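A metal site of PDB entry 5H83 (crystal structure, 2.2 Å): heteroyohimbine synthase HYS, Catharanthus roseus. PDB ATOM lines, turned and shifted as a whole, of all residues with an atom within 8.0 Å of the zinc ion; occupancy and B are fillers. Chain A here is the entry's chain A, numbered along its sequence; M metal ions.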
ATOM      1  N   GLY A  50      15.288   7.985   5.763  1.00  0.00           N
ATOM      2  CA  GLY A  50      13.985   8.566   5.491  1.00  0.00           C
ATOM      3  C   GLY A  50      12.859   7.606   5.828  1.00  0.00           C
ATOM      4  O   GLY A  50      13.072   6.397   5.936  1.00  0.00           O
ATOM      5  N   THR A  51      11.670   8.145   6.064  1.00  0.00           N
ATOM      6  CA  THR A  51      10.479   7.337   6.155  1.00  0.00           C
ATOM      7  C   THR A  51       9.313   8.135   5.602  1.00  0.00           C
ATOM      8  O   THR A  51       9.459   9.287   5.221  1.00  0.00           O
ATOM      9  CB  THR A  51      10.219   6.801   7.570  1.00  0.00           C
ATOM     10  OG1 THR A  51       9.116   5.892   7.521  1.00  0.00           O
ATOM     11  CG2 THR A  51       9.927   7.920   8.562  1.00  0.00           C
ATOM     12  N   CYS A  52       8.163   7.478   5.513  1.00  0.00           N
ATOM     13  CA  CYS A  52       7.022   7.954   4.715  1.00  0.00           C
ATOM     14  C   CYS A  52       5.827   7.040   4.923  1.00  0.00           C
ATOM     15  O   CYS A  52       5.944   6.053   5.661  1.00  0.00           O
ATOM     16  CB  CYS A  52       7.379   7.930   3.229  1.00  0.00           C
ATOM     17  SG  CYS A  52       7.739   6.255   2.645  1.00  0.00           S
ATOM     18  N   ASN A  53       4.709   7.325   4.269  1.00  0.00           N
ATOM     19  CA  ASN A  53       3.453   6.576   4.429  1.00  0.00           C
ATOM     20  C   ASN A  53       3.526   5.072   4.115  1.00  0.00           C
ATOM     21  O   ASN A  53       2.782   4.263   4.706  1.00  0.00           O
ATOM     22  CB  ASN A  53       2.359   7.192   3.575  1.00  0.00           C
ATOM     23  CG  ASN A  53       1.025   6.562   3.808  1.00  0.00           C
ATOM     24  OD1 ASN A  53       0.546   6.502   4.933  1.00  0.00           O
ATOM     25  ND2 ASN A  53       0.410   6.063   2.752  1.00  0.00           N
ATOM     26  N   TYR A  54       4.384   4.719   3.180  1.00  0.00           N
ATOM     27  CA  TYR A  54       4.644   3.332   2.873  1.00  0.00           C
ATOM     28  C   TYR A  54       5.061   2.521   4.125  1.00  0.00           C
ATOM     29  O   TYR A  54       4.593   1.393   4.326  1.00  0.00           O
ATOM     30  CB  TYR A  54       5.678   3.237   1.729  1.00  0.00           C
ATOM     31  CG  TYR A  54       6.205   1.867   1.538  1.00  0.00           C
ATOM     32  CD1 TYR A  54       5.596   0.959   0.659  1.00  0.00           C
ATOM     33  CD2 TYR A  54       7.288   1.422   2.294  1.00  0.00           C
ATOM     34  CE1 TYR A  54       6.084  -0.344   0.521  1.00  0.00           C
ATOM     35  CE2 TYR A  54       7.785   0.137   2.168  1.00  0.00           C
ATOM     36  CZ  TYR A  54       7.192  -0.741   1.284  1.00  0.00           C
ATOM     37  OH  TYR A  54       7.720  -2.005   1.191  1.00  0.00           O
ATOM     38  N   ASP A  55       5.927   3.077   4.969  1.00  0.00           N
ATOM     39  CA  ASP A  55       6.342   2.395   6.188  1.00  0.00           C
ATOM     40  C   ASP A  55       5.208   2.309   7.221  1.00  0.00           C
ATOM     41  O   ASP A  55       5.126   1.315   7.972  1.00  0.00           O
ATOM     42  CB  ASP A  55       7.556   3.070   6.826  1.00  0.00           C
ATOM     43  CG  ASP A  55       8.822   2.854   6.040  1.00  0.00           C
ATOM     44  OD1 ASP A  55       8.899   1.875   5.253  1.00  0.00           O
ATOM     45  OD2 ASP A  55       9.752   3.663   6.210  1.00  0.00           O
ATOM     46  N   GLY A  73      13.226   0.854   6.174  1.00  0.00           N
ATOM     47  CA  GLY A  73      14.393   1.598   5.692  1.00  0.00           C
ATOM     48  C   GLY A  73      14.637   1.342   4.246  1.00  0.00           C
ATOM     49  O   GLY A  73      15.470   0.520   3.919  1.00  0.00           O
ATOM     50  N   HIS A  74      13.925   2.081   3.394  1.00  0.00           N
ATOM     51  CA  HIS A  74      14.048   1.957   1.948  1.00  0.00           C
ATOM     52  C   HIS A  74      14.619   3.228   1.334  1.00  0.00           C
ATOM     53  O   HIS A  74      14.617   3.406   0.119  1.00  0.00           O
ATOM     54  CB  HIS A  74      12.695   1.583   1.298  1.00  0.00           C
ATOM     55  CG  HIS A  74      11.611   2.584   1.552  1.00  0.00           C
ATOM     56  ND1 HIS A  74      10.839   2.560   2.688  1.00  0.00           N
ATOM     57  CD2 HIS A  74      11.221   3.665   0.845  1.00  0.00           C
ATOM     58  CE1 HIS A  74      10.009   3.577   2.679  1.00  0.00           C
ATOM     59  NE2 HIS A  74      10.210   4.269   1.568  1.00  0.00           N
ATOM     60  N   GLU A  75      15.113   4.109   2.187  1.00  0.00           N
ATOM     61  CA  GLU A  75      15.650   5.389   1.735  1.00  0.00           C
ATOM     62  C   GLU A  75      16.651   5.775   2.786  1.00  0.00           C
ATOM     63  O   GLU A  75      16.266   6.269   3.835  1.00  0.00           O
ATOM     64  CB  GLU A  75      14.557   6.486   1.559  1.00  0.00           C
ATOM     65  CG  GLU A  75      13.222   6.276   2.301  1.00  0.00           C
ATOM     66  CD  GLU A  75      12.303   7.524   2.319  1.00  0.00           C
ATOM     67  OE1 GLU A  75      12.795   8.680   2.215  1.00  0.00           O
ATOM     68  OE2 GLU A  75      11.063   7.366   2.454  1.00  0.00           O
ATOM     69  N   VAL A 160      18.203  12.518   1.468  1.00  0.00           N
ATOM     70  CA  VAL A 160      17.817  11.093   1.536  1.00  0.00           C
ATOM     71  C   VAL A 160      16.411  10.788   0.982  1.00  0.00           C
ATOM     72  O   VAL A 160      16.275   9.804   0.264  1.00  0.00           O
ATOM     73  CB  VAL A 160      18.050  10.452   2.946  1.00  0.00           C
ATOM     74  CG1 VAL A 160      17.143  11.019   4.034  1.00  0.00           C
ATOM     75  CG2 VAL A 160      17.934   8.930   2.897  1.00  0.00           C
ATOM     76  N   PRO A 161      15.397  11.663   1.220  1.00  0.00           N
ATOM     77  CA  PRO A 161      14.093  11.351   0.590  1.00  0.00           C
ATOM     78  C   PRO A 161      14.068  11.375  -0.945  1.00  0.00           C
ATOM     79  O   PRO A 161      13.092  10.932  -1.514  1.00  0.00           O
ATOM     80  CB  PRO A 161      13.124  12.415   1.165  1.00  0.00           C
ATOM     81  CG  PRO A 161      13.825  13.011   2.351  1.00  0.00           C
ATOM     82  CD  PRO A 161      15.307  12.906   2.003  1.00  0.00           C
ATOM     83  N   LEU A 163      15.686   9.426  -2.663  1.00  0.00           N
ATOM     84  CA  LEU A 163      15.687   7.984  -2.994  1.00  0.00           C
ATOM     85  C   LEU A 163      14.322   7.326  -2.985  1.00  0.00           C
ATOM     86  O   LEU A 163      14.208   6.170  -3.433  1.00  0.00           O
ATOM     87  CB  LEU A 163      16.626   7.213  -2.062  1.00  0.00           C
ATOM     88  CG  LEU A 163      18.074   7.669  -2.188  1.00  0.00           C
ATOM     89  CD1 LEU A 163      18.874   7.115  -1.019  1.00  0.00           C
ATOM     90  CD2 LEU A 163      18.630   7.254  -3.555  1.00  0.00           C
ATOM     91  N   CYS A 164      13.317   8.027  -2.449  1.00  0.00           N
ATOM     92  CA  CYS A 164      11.937   7.581  -2.409  1.00  0.00           C
ATOM     93  C   CYS A 164      11.016   8.545  -3.177  1.00  0.00           C
ATOM     94  O   CYS A 164      10.537   8.196  -4.290  1.00  0.00           O
ATOM     95  CB  CYS A 164      11.499   7.411  -0.966  1.00  0.00           C
ATOM     96  SG  CYS A 164       9.786   6.947  -0.706  1.00  0.00           S
ATOM     97  N   ALA A 165      10.755   9.726  -2.602  1.00  0.00           N
ATOM     98  CA  ALA A 165       9.855  10.713  -3.224  1.00  0.00           C
ATOM     99  C   ALA A 165      10.481  11.311  -4.479  1.00  0.00           C
ATOM    100  O   ALA A 165       9.796  11.558  -5.456  1.00  0.00           O
ATOM    101  CB  ALA A 165       9.496  11.807  -2.244  1.00  0.00           C
ATOM    102  N   THR A 168      10.469   8.856  -7.653  1.00  0.00           N
ATOM    103  CA  THR A 168       9.071   8.718  -8.032  1.00  0.00           C
ATOM    104  C   THR A 168       8.555   9.801  -8.970  1.00  0.00           C
ATOM    105  O   THR A 168       7.746   9.494  -9.844  1.00  0.00           O
ATOM    106  CB  THR A 168       8.211   8.647  -6.768  1.00  0.00           C
ATOM    107  OG1 THR A 168       8.633   7.509  -6.023  1.00  0.00           O
ATOM    108  CG2 THR A 168       6.750   8.535  -7.073  1.00  0.00           C
ATOM    109  N   LEU A 193       5.521  14.340  -2.438  1.00  0.00           N
ATOM    110  CA  LEU A 193       5.872  14.114  -3.822  1.00  0.00           C
ATOM    111  C   LEU A 193       5.878  15.434  -4.631  1.00  0.00           C
ATOM    112  O   LEU A 193       6.826  15.711  -5.367  1.00  0.00           O
ATOM    113  CB  LEU A 193       4.912  13.114  -4.464  1.00  0.00           C
ATOM    114  CG  LEU A 193       4.882  11.709  -3.835  1.00  0.00           C
ATOM    115  CD1 LEU A 193       4.054  10.783  -4.708  1.00  0.00           C
ATOM    116  CD2 LEU A 193       6.284  11.138  -3.663  1.00  0.00           C
ATOM    117  N   ARG A 346       8.816  15.484   4.805  1.00  0.00           N
ATOM    118  CA  ARG A 346       9.238  14.105   5.035  1.00  0.00           C
ATOM    119  C   ARG A 346      10.025  13.996   6.344  1.00  0.00           C
ATOM    120  O   ARG A 346      10.829  14.853   6.647  1.00  0.00           O
ATOM    121  CB  ARG A 346      10.073  13.577   3.855  1.00  0.00           C
ATOM    122  CG  ARG A 346       9.261  13.198   2.605  1.00  0.00           C
ATOM    123  CD  ARG A 346       8.318  12.037   2.883  1.00  0.00           C
ATOM    124  NE  ARG A 346       7.697  11.436   1.699  1.00  0.00           N
ATOM    125  CZ  ARG A 346       8.235  10.484   0.915  1.00  0.00           C
ATOM    126  NH1 ARG A 346       9.484   9.990   1.123  1.00  0.00           N
ATOM    127  NH2 ARG A 346       7.521  10.032  -0.107  1.00  0.00           N
ATOM    128  N   PHE A 347       9.740  12.950   7.121  1.00  0.00           N
ATOM    129  CA  PHE A 347      10.596  12.597   8.246  1.00  0.00           C
ATOM    130  C   PHE A 347      11.925  11.974   7.824  1.00  0.00           C
ATOM    131  O   PHE A 347      11.971  11.143   6.928  1.00  0.00           O
ATOM    132  CB  PHE A 347       9.878  11.669   9.207  1.00  0.00           C
ATOM    133  CG  PHE A 347       8.831  12.359  10.016  1.00  0.00           C
ATOM    134  CD1 PHE A 347       9.197  13.305  10.979  1.00  0.00           C
ATOM    135  CD2 PHE A 347       7.493  12.087   9.816  1.00  0.00           C
ATOM    136  CE1 PHE A 347       8.228  13.961  11.752  1.00  0.00           C
ATOM    137  CE2 PHE A 347       6.516  12.725  10.577  1.00  0.00           C
ATOM    138  CZ  PHE A 347       6.887  13.663  11.541  1.00  0.00           C
HETATM  139 ZN    ZN M   1       9.724   6.214   1.479  1.00  0.00          ZN
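A ring nitrogen (ND1) of His 74 lies close to the side-chain carboxylate (OD1) of Asp 55, at 3.3 Å. The guanidinium group (NH1) of Arg 346 is in salt-bridge range of the side-chain carboxylate (OE1) of Glu 75. The backbone NH (N) of Gly 50 lies within hydrogen-bond range of the backbone carbonyl oxygen (O) of Glu 75. The side-chain sulfur (SG) of Cys 52 lies close to the backbone NH (N) of Tyr 54. SG of Cys 164 lies close to NH1 of Arg 346, 3.6 Å away. The side-chain hydroxyl (OG1) of Thr 168 lies within hydrogen-bond range of the backbone carbonyl oxygen (O) of Cys 164, at 2.7 Å.
The zinc ion is bound by a ring nitrogen (NE2) of His 74 (2.0 Å), the side-chain carboxylate (OE2) of Glu 75 (2.0 Å), the side-chain sulfur (SG) of Cys 52 (2.3 Å) and the side-chain sulfur (SG) of Cys 164 (2.3 Å).
Merely in contact with the zinc ion: Arg 346 (3.8 Å). Five residues have an atom within 4 Å of the zinc ion: Cys 52, His 74, Glu 75, Cys 164 and Arg 346. The nearest printed residue that does not touch the zinc ion is Thr 51 (4.6 Å).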
